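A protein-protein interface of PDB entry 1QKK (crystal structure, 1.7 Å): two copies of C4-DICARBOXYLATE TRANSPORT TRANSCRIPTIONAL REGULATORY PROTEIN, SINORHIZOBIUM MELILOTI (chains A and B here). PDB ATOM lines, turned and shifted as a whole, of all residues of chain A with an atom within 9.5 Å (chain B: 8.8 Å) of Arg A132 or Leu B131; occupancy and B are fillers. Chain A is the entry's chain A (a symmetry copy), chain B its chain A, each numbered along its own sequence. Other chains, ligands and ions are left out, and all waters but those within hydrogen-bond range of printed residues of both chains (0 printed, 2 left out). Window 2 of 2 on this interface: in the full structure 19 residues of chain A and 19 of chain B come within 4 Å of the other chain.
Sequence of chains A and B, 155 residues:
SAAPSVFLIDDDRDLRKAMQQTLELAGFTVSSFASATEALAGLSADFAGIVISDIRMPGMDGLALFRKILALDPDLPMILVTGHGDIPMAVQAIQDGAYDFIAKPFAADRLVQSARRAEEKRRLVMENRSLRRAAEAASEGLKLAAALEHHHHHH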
ATOM      1  N   LEU A 124       4.715 -15.943  32.578  1.00  0.00           N
ATOM      2  CA  LEU A 124       5.547 -16.341  31.448  1.00  0.00           C
ATOM      3  C   LEU A 124       6.055 -17.773  31.613  1.00  0.00           C
ATOM      4  O   LEU A 124       6.085 -18.545  30.653  1.00  0.00           O
ATOM      5  CB  LEU A 124       6.731 -15.383  31.300  1.00  0.00           C
ATOM      6  CG  LEU A 124       6.403 -14.000  30.730  1.00  0.00           C
ATOM      7  CD1 LEU A 124       7.607 -13.084  30.869  1.00  0.00           C
ATOM      8  CD2 LEU A 124       5.993 -14.137  29.271  1.00  0.00           C
ATOM      9  N   VAL A 125       6.459 -18.126  32.829  1.00  0.00           N
ATOM     10  CA  VAL A 125       6.953 -19.471  33.096  1.00  0.00           C
ATOM     11  C   VAL A 125       5.853 -20.509  32.869  1.00  0.00           C
ATOM     12  O   VAL A 125       6.091 -21.551  32.252  1.00  0.00           O
ATOM     13  CB  VAL A 125       7.483 -19.590  34.544  1.00  0.00           C
ATOM     14  CG1 VAL A 125       7.733 -21.048  34.903  1.00  0.00           C
ATOM     15  CG2 VAL A 125       8.775 -18.799  34.681  1.00  0.00           C
ATOM     16  N   MET A 126       4.648 -20.227  33.355  1.00  0.00           N
ATOM     17  CA  MET A 126       3.553 -21.176  33.180  1.00  0.00           C
ATOM     18  C   MET A 126       3.139 -21.269  31.711  1.00  0.00           C
ATOM     19  O   MET A 126       2.769 -22.346  31.230  1.00  0.00           O
ATOM     20  CB  MET A 126       2.360 -20.793  34.068  1.00  0.00           C
ATOM     21  CG  MET A 126       2.663 -20.836  35.584  1.00  0.00           C
ATOM     22  SD  MET A 126       3.393 -22.382  36.224  1.00  0.00           S
ATOM     23  CE  MET A 126       1.917 -23.267  36.737  1.00  0.00           C
ATOM     24  N   GLU A 127       3.212 -20.151  30.992  1.00  0.00           N
ATOM     25  CA  GLU A 127       2.871 -20.147  29.571  1.00  0.00           C
ATOM     26  C   GLU A 127       3.902 -20.975  28.806  1.00  0.00           C
ATOM     27  O   GLU A 127       3.560 -21.723  27.889  1.00  0.00           O
ATOM     28  CB  GLU A 127       2.851 -18.717  29.023  1.00  0.00           C
ATOM     29  CG  GLU A 127       1.579 -17.944  29.337  1.00  0.00           C
ATOM     30  CD  GLU A 127       1.615 -16.522  28.803  1.00  0.00           C
ATOM     31  OE1 GLU A 127       2.130 -16.322  27.682  1.00  0.00           O
ATOM     32  OE2 GLU A 127       1.117 -15.608  29.499  1.00  0.00           O
ATOM     33  N   ASN A 128       5.166 -20.831  29.193  1.00  0.00           N
ATOM     34  CA  ASN A 128       6.256 -21.566  28.564  1.00  0.00           C
ATOM     35  C   ASN A 128       6.049 -23.063  28.761  1.00  0.00           C
ATOM     36  O   ASN A 128       6.184 -23.846  27.820  1.00  0.00           O
ATOM     37  CB  ASN A 128       7.596 -21.127  29.170  1.00  0.00           C
ATOM     38  CG  ASN A 128       8.782 -21.899  28.610  1.00  0.00           C
ATOM     39  OD1 ASN A 128       9.030 -23.048  28.987  1.00  0.00           O
ATOM     40  ND2 ASN A 128       9.519 -21.269  27.701  1.00  0.00           N
ATOM     41  N   ARG A 129       5.707 -23.457  29.983  1.00  0.00           N
ATOM     42  CA  ARG A 129       5.483 -24.863  30.288  1.00  0.00           C
ATOM     43  C   ARG A 129       4.284 -25.401  29.526  1.00  0.00           C
ATOM     44  O   ARG A 129       4.314 -26.526  29.021  1.00  0.00           O
ATOM     45  CB  ARG A 129       5.283 -25.050  31.793  1.00  0.00           C
ATOM     46  CG  ARG A 129       6.550 -24.791  32.591  1.00  0.00           C
ATOM     47  CD  ARG A 129       6.331 -24.900  34.090  1.00  0.00           C
ATOM     48  NE  ARG A 129       7.564 -24.595  34.811  1.00  0.00           N
ATOM     49  CZ  ARG A 129       7.658 -24.492  36.133  1.00  0.00           C
ATOM     50  NH1 ARG A 129       6.588 -24.672  36.895  1.00  0.00           N
ATOM     51  NH2 ARG A 129       8.825 -24.208  36.692  1.00  0.00           N
ATOM     52  N   SER A 130       3.234 -24.593  29.437  1.00  0.00           N
ATOM     53  CA  SER A 130       2.023 -24.982  28.724  1.00  0.00           C
ATOM     54  C   SER A 130       2.322 -25.216  27.246  1.00  0.00           C
ATOM     55  O   SER A 130       1.814 -26.163  26.643  1.00  0.00           O
ATOM     56  CB  SER A 130       0.955 -23.898  28.865  1.00  0.00           C
ATOM     57  OG  SER A 130      -0.169 -24.190  28.052  1.00  0.00           O
ATOM     58  N   LEU A 131       3.145 -24.349  26.666  1.00  0.00           N
ATOM     59  CA  LEU A 131       3.510 -24.470  25.262  1.00  0.00           C
ATOM     60  C   LEU A 131       4.351 -25.719  25.020  1.00  0.00           C
ATOM     61  O   LEU A 131       4.161 -26.421  24.024  1.00  0.00           O
ATOM     62  CB  LEU A 131       4.273 -23.225  24.801  1.00  0.00           C
ATOM     63  CG  LEU A 131       3.414 -21.967  24.622  1.00  0.00           C
ATOM     64  CD1 LEU A 131       4.294 -20.738  24.430  1.00  0.00           C
ATOM     65  CD2 LEU A 131       2.495 -22.162  23.429  1.00  0.00           C
ATOM     66  N   ARG A 132       5.280 -26.001  25.930  1.00  0.00           N
ATOM     67  CA  ARG A 132       6.126 -27.182  25.787  1.00  0.00           C
ATOM     68  C   ARG A 132       5.298 -28.451  25.927  1.00  0.00           C
ATOM     69  O   ARG A 132       5.546 -29.437  25.233  1.00  0.00           O
ATOM     70  CB  ARG A 132       7.254 -27.170  26.823  1.00  0.00           C
ATOM     71  CG  ARG A 132       8.292 -26.088  26.572  1.00  0.00           C
ATOM     72  CD  ARG A 132       9.444 -26.166  27.563  1.00  0.00           C
ATOM     73  NE  ARG A 132      10.356 -25.036  27.411  1.00  0.00           N
ATOM     74  CZ  ARG A 132      11.152 -24.844  26.363  1.00  0.00           C
ATOM     75  NH1 ARG A 132      11.162 -25.714  25.362  1.00  0.00           N
ATOM     76  NH2 ARG A 132      11.932 -23.771  26.308  1.00  0.00           N
ATOM     77  N   ARG A 133       4.313 -28.427  26.822  1.00  0.00           N
ATOM     78  CA  ARG A 133       3.438 -29.580  27.019  1.00  0.00           C
ATOM     79  C   ARG A 133       2.706 -29.870  25.714  1.00  0.00           C
ATOM     80  O   ARG A 133       2.621 -31.019  25.274  1.00  0.00           O
ATOM     81  CB  ARG A 133       2.398 -29.297  28.110  1.00  0.00           C
ATOM     82  CG  ARG A 133       2.699 -29.900  29.474  1.00  0.00           C
ATOM     83  CD  ARG A 133       3.953 -29.312  30.090  1.00  0.00           C
ATOM     84  NE  ARG A 133       4.159 -29.796  31.453  1.00  0.00           N
ATOM     85  CZ  ARG A 133       5.206 -29.480  32.208  1.00  0.00           C
ATOM     86  NH1 ARG A 133       6.148 -28.673  31.735  1.00  0.00           N
ATOM     87  NH2 ARG A 133       5.311 -29.971  33.435  1.00  0.00           N
ATOM     88  N   ALA A 134       2.179 -28.815  25.100  1.00  0.00           N
ATOM     89  CA  ALA A 134       1.442 -28.939  23.848  1.00  0.00           C
ATOM     90  C   ALA A 134       2.316 -29.469  22.716  1.00  0.00           C
ATOM     91  O   ALA A 134       1.867 -30.284  21.908  1.00  0.00           O
ATOM     92  CB  ALA A 134       0.848 -27.590  23.459  1.00  0.00           C
ATOM     93  N   ALA A 135       3.560 -29.007  22.656  1.00  0.00           N
ATOM     94  CA  ALA A 135       4.482 -29.446  21.615  1.00  0.00           C
ATOM     95  C   ALA A 135       4.770 -30.939  21.743  1.00  0.00           C
ATOM     96  O   ALA A 135       4.784 -31.666  20.747  1.00  0.00           O
ATOM     97  CB  ALA A 135       5.781 -28.655  21.699  1.00  0.00           C
ATOM     98  N   GLU A 136       5.002 -31.391  22.971  1.00  0.00           N
ATOM     99  CA  GLU A 136       5.287 -32.798  23.220  1.00  0.00           C
ATOM    100  C   GLU A 136       4.048 -33.649  22.967  1.00  0.00           C
ATOM    101  O   GLU A 136       4.144 -34.767  22.460  1.00  0.00           O
ATOM    102  CB  GLU A 136       5.777 -32.994  24.658  1.00  0.00           C
ATOM    103  CG  GLU A 136       7.101 -32.304  24.951  1.00  0.00           C
ATOM    104  CD  GLU A 136       7.567 -32.503  26.383  1.00  0.00           C
ATOM    105  OE1 GLU A 136       6.836 -32.090  27.310  1.00  0.00           O
ATOM    106  OE2 GLU A 136       8.664 -33.070  26.581  1.00  0.00           O
ATOM    107  N   ALA A 137       2.883 -33.114  23.317  1.00  0.00           N
ATOM    108  CA  ALA A 137       1.627 -33.825  23.115  1.00  0.00           C
ATOM    109  C   ALA A 137       1.384 -34.019  21.620  1.00  0.00           C
ATOM    110  O   ALA A 137       0.933 -35.079  21.185  1.00  0.00           O
ATOM    111  CB  ALA A 137       0.479 -33.045  23.737  1.00  0.00           C
ATOM    112  N   ALA A 138       1.687 -32.986  20.839  1.00  0.00           N
ATOM    113  CA  ALA A 138       1.510 -33.048  19.393  1.00  0.00           C
ATOM    114  C   ALA A 138       2.534 -34.001  18.791  1.00  0.00           C
ATOM    115  O   ALA A 138       2.211 -34.813  17.921  1.00  0.00           O
ATOM    116  CB  ALA A 138       1.672 -31.661  18.788  1.00  0.00           C
ATOM    117  N   SER A 139       3.771 -33.896  19.263  1.00  0.00           N
ATOM    118  CA  SER A 139       4.854 -34.739  18.777  1.00  0.00           C
ATOM    119  C   SER A 139       4.568 -36.218  19.033  1.00  0.00           C
ATOM    120  O   SER A 139       4.828 -37.062  18.175  1.00  0.00           O
ATOM    121  CB  SER A 139       6.169 -34.337  19.448  1.00  0.00           C
ATOM    122  OG  SER A 139       7.266 -35.043  18.895  1.00  0.00           O
ATOM    123  N   GLU A 140       4.032 -36.529  20.210  1.00  0.00           N
ATOM    124  CA  GLU A 140       3.715 -37.913  20.551  1.00  0.00           C
ATOM    125  C   GLU A 140       2.565 -38.440  19.702  1.00  0.00           C
ATOM    126  O   GLU A 140       2.590 -39.587  19.256  1.00  0.00           O
ATOM    127  CB  GLU A 140       3.349 -38.040  22.032  1.00  0.00           C
ATOM    128  CG  GLU A 140       4.529 -37.909  22.981  1.00  0.00           C
ATOM    129  CD  GLU A 140       4.152 -38.198  24.423  1.00  0.00           C
ATOM    130  OE1 GLU A 140       3.681 -39.323  24.703  1.00  0.00           O
ATOM    131  OE2 GLU A 140       4.327 -37.301  25.277  1.00  0.00           O
ATOM    132  N   ARG B 123      14.330 -13.093  28.327  1.00  0.00           N
ATOM    133  CA  ARG B 123      14.639 -14.464  27.924  1.00  0.00           C
ATOM    134  C   ARG B 123      13.358 -15.289  27.816  1.00  0.00           C
ATOM    135  O   ARG B 123      13.171 -16.050  26.857  1.00  0.00           O
ATOM    136  CB  ARG B 123      15.588 -15.114  28.934  1.00  0.00           C
ATOM    137  CG  ARG B 123      16.005 -16.530  28.558  1.00  0.00           C
ATOM    138  CD  ARG B 123      16.946 -17.137  29.586  1.00  0.00           C
ATOM    139  NE  ARG B 123      16.289 -17.358  30.872  1.00  0.00           N
ATOM    140  CZ  ARG B 123      16.550 -16.669  31.979  1.00  0.00           C
ATOM    141  NH1 ARG B 123      17.461 -15.705  31.968  1.00  0.00           N
ATOM    142  NH2 ARG B 123      15.899 -16.944  33.101  1.00  0.00           N
ATOM    143  N   LEU B 124      12.473 -15.137  28.797  1.00  0.00           N
ATOM    144  CA  LEU B 124      11.207 -15.863  28.798  1.00  0.00           C
ATOM    145  C   LEU B 124      10.317 -15.423  27.637  1.00  0.00           C
ATOM    146  O   LEU B 124       9.670 -16.249  26.991  1.00  0.00           O
ATOM    147  CB  LEU B 124      10.476 -15.647  30.125  1.00  0.00           C
ATOM    148  CG  LEU B 124      11.048 -16.396  31.331  1.00  0.00           C
ATOM    149  CD1 LEU B 124      10.388 -15.904  32.608  1.00  0.00           C
ATOM    150  CD2 LEU B 124      10.828 -17.892  31.151  1.00  0.00           C
ATOM    151  N   VAL B 125      10.279 -14.121  27.374  1.00  0.00           N
ATOM    152  CA  VAL B 125       9.468 -13.596  26.282  1.00  0.00           C
ATOM    153  C   VAL B 125       9.964 -14.125  24.936  1.00  0.00           C
ATOM    154  O   VAL B 125       9.164 -14.537  24.091  1.00  0.00           O
ATOM    155  CB  VAL B 125       9.489 -12.050  26.269  1.00  0.00           C
ATOM    156  CG1 VAL B 125       8.881 -11.520  24.978  1.00  0.00           C
ATOM    157  CG2 VAL B 125       8.706 -11.519  27.460  1.00  0.00           C
ATOM    158  N   MET B 126      11.277 -14.124  24.734  1.00  0.00           N
ATOM    159  CA  MET B 126      11.820 -14.609  23.469  1.00  0.00           C
ATOM    160  C   MET B 126      11.616 -16.118  23.329  1.00  0.00           C
ATOM    161  O   MET B 126      11.377 -16.619  22.224  1.00  0.00           O
ATOM    162  CB  MET B 126      13.304 -14.237  23.339  1.00  0.00           C
ATOM    163  CG  MET B 126      13.572 -12.714  23.311  1.00  0.00           C
ATOM    164  SD  MET B 126      12.620 -11.744  22.092  1.00  0.00           S
ATOM    165  CE  MET B 126      13.760 -11.729  20.704  1.00  0.00           C
ATOM    166  N   GLU B 127      11.694 -16.843  24.442  1.00  0.00           N
ATOM    167  CA  GLU B 127      11.480 -18.288  24.415  1.00  0.00           C
ATOM    168  C   GLU B 127      10.020 -18.571  24.064  1.00  0.00           C
ATOM    169  O   GLU B 127       9.718 -19.493  23.304  1.00  0.00           O
ATOM    170  CB  GLU B 127      11.811 -18.910  25.774  1.00  0.00           C
ATOM    171  CG  GLU B 127      13.297 -19.129  26.017  1.00  0.00           C
ATOM    172  CD  GLU B 127      13.582 -19.718  27.388  1.00  0.00           C
ATOM    173  OE1 GLU B 127      12.807 -20.592  27.833  1.00  0.00           O
ATOM    174  OE2 GLU B 127      14.588 -19.315  28.015  1.00  0.00           O
ATOM    175  N   ASN B 128       9.121 -17.769  24.627  1.00  0.00           N
ATOM    176  CA  ASN B 128       7.692 -17.911  24.375  1.00  0.00           C
ATOM    177  C   ASN B 128       7.406 -17.693  22.894  1.00  0.00           C
ATOM    178  O   ASN B 128       6.672 -18.463  22.275  1.00  0.00           O
ATOM    179  CB  ASN B 128       6.911 -16.900  25.226  1.00  0.00           C
ATOM    180  CG  ASN B 128       5.412 -16.941  24.969  1.00  0.00           C
ATOM    181  OD1 ASN B 128       4.923 -16.418  23.965  1.00  0.00           O
ATOM    182  ND2 ASN B 128       4.675 -17.570  25.879  1.00  0.00           N
ATOM    183  N   ARG B 129       7.999 -16.648  22.326  1.00  0.00           N
ATOM    184  CA  ARG B 129       7.799 -16.341  20.917  1.00  0.00           C
ATOM    185  C   ARG B 129       8.366 -17.440  20.034  1.00  0.00           C
ATOM    186  O   ARG B 129       7.757 -17.817  19.030  1.00  0.00           O
ATOM    187  CB  ARG B 129       8.445 -14.998  20.573  1.00  0.00           C
ATOM    188  CG  ARG B 129       7.733 -13.821  21.218  1.00  0.00           C
ATOM    189  CD  ARG B 129       8.420 -12.495  20.940  1.00  0.00           C
ATOM    190  NE  ARG B 129       7.726 -11.406  21.621  1.00  0.00           N
ATOM    191  CZ  ARG B 129       8.156 -10.149  21.664  1.00  0.00           C
ATOM    192  NH1 ARG B 129       9.288  -9.809  21.064  1.00  0.00           N
ATOM    193  NH2 ARG B 129       7.452  -9.232  22.312  1.00  0.00           N
ATOM    194  N   SER B 130       9.529 -17.958  20.415  1.00  0.00           N
ATOM    195  CA  SER B 130      10.177 -19.026  19.663  1.00  0.00           C
ATOM    196  C   SER B 130       9.305 -20.277  19.649  1.00  0.00           C
ATOM    197  O   SER B 130       9.188 -20.952  18.624  1.00  0.00           O
ATOM    198  CB  SER B 130      11.536 -19.356  20.280  1.00  0.00           C
ATOM    199  OG  SER B 130      12.108 -20.493  19.657  1.00  0.00           O
ATOM    200  N   LEU B 131       8.698 -20.587  20.789  1.00  0.00           N
ATOM    201  CA  LEU B 131       7.835 -21.755  20.899  1.00  0.00           C
ATOM    202  C   LEU B 131       6.576 -21.588  20.053  1.00  0.00           C
ATOM    203  O   LEU B 131       6.132 -22.532  19.396  1.00  0.00           O
ATOM    204  CB  LEU B 131       7.457 -22.002  22.362  1.00  0.00           C
ATOM    205  CG  LEU B 131       8.583 -22.568  23.236  1.00  0.00           C
ATOM    206  CD1 LEU B 131       8.195 -22.522  24.708  1.00  0.00           C
ATOM    207  CD2 LEU B 131       8.877 -23.993  22.801  1.00  0.00           C
ATOM    208  N   ARG B 132       6.001 -20.388  20.065  1.00  0.00           N
ATOM    209  CA  ARG B 132       4.799 -20.132  19.279  1.00  0.00           C
ATOM    210  C   ARG B 132       5.109 -20.205  17.791  1.00  0.00           C
ATOM    211  O   ARG B 132       4.294 -20.690  17.008  1.00  0.00           O
ATOM    212  CB  ARG B 132       4.203 -18.765  19.629  1.00  0.00           C
ATOM    213  CG  ARG B 132       3.605 -18.707  21.025  1.00  0.00           C
ATOM    214  CD  ARG B 132       2.939 -17.367  21.302  1.00  0.00           C
ATOM    215  NE  ARG B 132       2.503 -17.265  22.691  1.00  0.00           N
ATOM    216  CZ  ARG B 132       1.509 -17.970  23.223  1.00  0.00           C
ATOM    217  NH1 ARG B 132       0.830 -18.835  22.482  1.00  0.00           N
ATOM    218  NH2 ARG B 132       1.201 -17.821  24.507  1.00  0.00           N
ATOM    219  N   ARG B 133       6.288 -19.726  17.402  1.00  0.00           N
ATOM    220  CA  ARG B 133       6.702 -19.770  16.001  1.00  0.00           C
ATOM    221  C   ARG B 133       6.760 -21.226  15.553  1.00  0.00           C
ATOM    222  O   ARG B 133       6.264 -21.581  14.481  1.00  0.00           O
ATOM    223  CB  ARG B 133       8.091 -19.147  15.821  1.00  0.00           C
ATOM    224  CG  ARG B 133       8.106 -17.726  15.280  1.00  0.00           C
ATOM    225  CD  ARG B 133       7.456 -16.747  16.238  1.00  0.00           C
ATOM    226  NE  ARG B 133       7.595 -15.368  15.773  1.00  0.00           N
ATOM    227  CZ  ARG B 133       7.077 -14.315  16.394  1.00  0.00           C
ATOM    228  NH1 ARG B 133       6.383 -14.477  17.514  1.00  0.00           N
ATOM    229  NH2 ARG B 133       7.252 -13.098  15.896  1.00  0.00           N
ATOM    230  N   ALA B 134       7.371 -22.063  16.386  1.00  0.00           N
ATOM    231  CA  ALA B 134       7.513 -23.483  16.087  1.00  0.00           C
ATOM    232  C   ALA B 134       6.163 -24.186  15.980  1.00  0.00           C
ATOM    233  O   ALA B 134       5.968 -25.039  15.112  1.00  0.00           O
ATOM    234  CB  ALA B 134       8.367 -24.157  17.154  1.00  0.00           C
ATOM    235  N   ALA B 135       5.234 -23.830  16.861  1.00  0.00           N
ATOM    236  CA  ALA B 135       3.908 -24.437  16.850  1.00  0.00           C
ATOM    237  C   ALA B 135       3.172 -24.106  15.556  1.00  0.00           C
ATOM    238  O   ALA B 135       2.543 -24.976  14.948  1.00  0.00           O
ATOM    239  CB  ALA B 135       3.101 -23.953  18.048  1.00  0.00           C
ATOM    240  N   GLU B 136       3.252 -22.847  15.139  1.00  0.00           N
ATOM    241  CA  GLU B 136       2.592 -22.411  13.915  1.00  0.00           C
ATOM    242  C   GLU B 136       3.265 -23.027  12.694  1.00  0.00           C
ATOM    243  O   GLU B 136       2.601 -23.382  11.721  1.00  0.00           O
ATOM    244  CB  GLU B 136       2.616 -20.882  13.816  1.00  0.00           C
ATOM    245  CG  GLU B 136       1.827 -20.186  14.915  1.00  0.00           C
ATOM    246  CD  GLU B 136       1.868 -18.672  14.804  1.00  0.00           C
ATOM    247  OE1 GLU B 136       2.979 -18.100  14.866  1.00  0.00           O
ATOM    248  OE2 GLU B 136       0.791 -18.054  14.657  1.00  0.00           O
ATOM    249  N   ALA B 137       4.587 -23.157  12.752  1.00  0.00           N
ATOM    250  CA  ALA B 137       5.342 -23.741  11.651  1.00  0.00           C
ATOM    251  C   ALA B 137       4.946 -25.206  11.480  1.00  0.00           C
ATOM    252  O   ALA B 137       4.799 -25.695  10.359  1.00  0.00           O
ATOM    253  CB  ALA B 137       6.835 -23.630  11.925  1.00  0.00           C
ATOM    254  N   ALA B 138       4.773 -25.901  12.601  1.00  0.00           N
ATOM    255  CA  ALA B 138       4.384 -27.306  12.573  1.00  0.00           C
ATOM    256  C   ALA B 138       2.944 -27.430  12.093  1.00  0.00           C
ATOM    257  O   ALA B 138       2.620 -28.296  11.277  1.00  0.00           O
ATOM    258  CB  ALA B 138       4.523 -27.913  13.962  1.00  0.00           C
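NH2 of Arg B132 lies within salt-bridge range of OE1 of Glu A127, at 3.6 Å.
The side-chain amide nitrogen of Asn B128 lies within hydrogen-bond range of the side-chain carboxylate of Glu A127, 3.4 Å away.
The side-chain carboxylate (OE1) of Glu B127 is in hydrogen-bond range of the side-chain amide nitrogen (ND2) of Asn A128 (3.4 Å).
NH2 of Arg A132 lies within salt-bridge range of OE1 of Glu B127 (3.6 Å).
Of chain B, only Glu B127 (3.6 Å) and Leu B131 (3.8 Å) come within 4 Å of Arg A132.
Printed residues of chain A within 4 Å of Leu B124: Leu A124 (3.9 Å) and Val A125 (3.9 Å).
Printed residues of chain A within 4 Å of Val B125: Leu A124 (3.9 Å).
Of the printed residues of chain A, Asn B128 touches Glu A127 and Leu A131.
No residue of chain A comes within 4 Å of Ser B130.
Printed residues of chain A within 4 Å of Leu B131: Asn A128, Leu A131 and Arg A132.
Arg B133 touches none of the printed residues of chain A.
No residue of chain A comes within 4 Å of Ala B134.
The nearest printed residue of chain A that does not touch Leu B131 is Glu A127 (5.7 Å).
Leu A124 touches Leu B124 (CD1 to CB, 3.9 Å).
Leu A124 touches Val B125 (CD1 to CG2, 3.9 Å).
CG2 of Val A125 touches CD1 of Leu B124, at 3.9 Å.
CD1 of Leu B131 touches ND2 of Asn A128, 3.5 Å away.
CD1 of Leu A131 touches ND2 of Asn B128, 3.5 Å away.
Leu A131 touches Leu B131 (CD1 to CB, 3.98 Å).
CD2 of Leu A131 touches NH1 of Arg B132, at 3.8 Å.
Leu B131 touches Arg A132 (CD2 to NH1, 3.8 Å).
Printed residues of chain B that touch a printed residue of chain A: Leu B124, Val B125, Glu B127, Asn B128, Leu B131 and Arg B132.
Of the 17 printed residues of chain A, 6 touch a printed residue of chain B.
Among the printed residues, Asp or Glu carboxylates within 4 Å of a Lys or Arg side-chain nitrogen of the other chain: Glu A127 with Arg B132 (3.6 Å) and Arg A132 with Glu B127 (3.6 Å).
The side-chain amide oxygen (OD1) of Asn A128 is in hydrogen-bond range of the guanidinium group (NE) of Arg A132.
The side-chain amide oxygen of Asn B128 sits at hydrogen-bond distance from the guanidinium group of Arg B132, at 2.9 Å.
The guanidinium group of Arg B123 is in salt-bridge range of the side-chain carboxylate of Glu B127 (3.9 Å).
Leu A124 touches Val B125, and with the chains exchanged Val A125 touches Leu B124.
Glu A127 touches Asn B128, and with the chains exchanged Asn A128 touches Glu B127.
Glu A127 touches Arg B132, and with the chains exchanged Arg A132 touches Glu B127.
Asn A128 touches Leu B131, and with the chains exchanged Leu A131 touches Asn B128.
15 positions are printed for both chains.
Of the 12 pairs that touch across the chains among the printed residues, 12 have their exchanged pair printed and touching as well.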
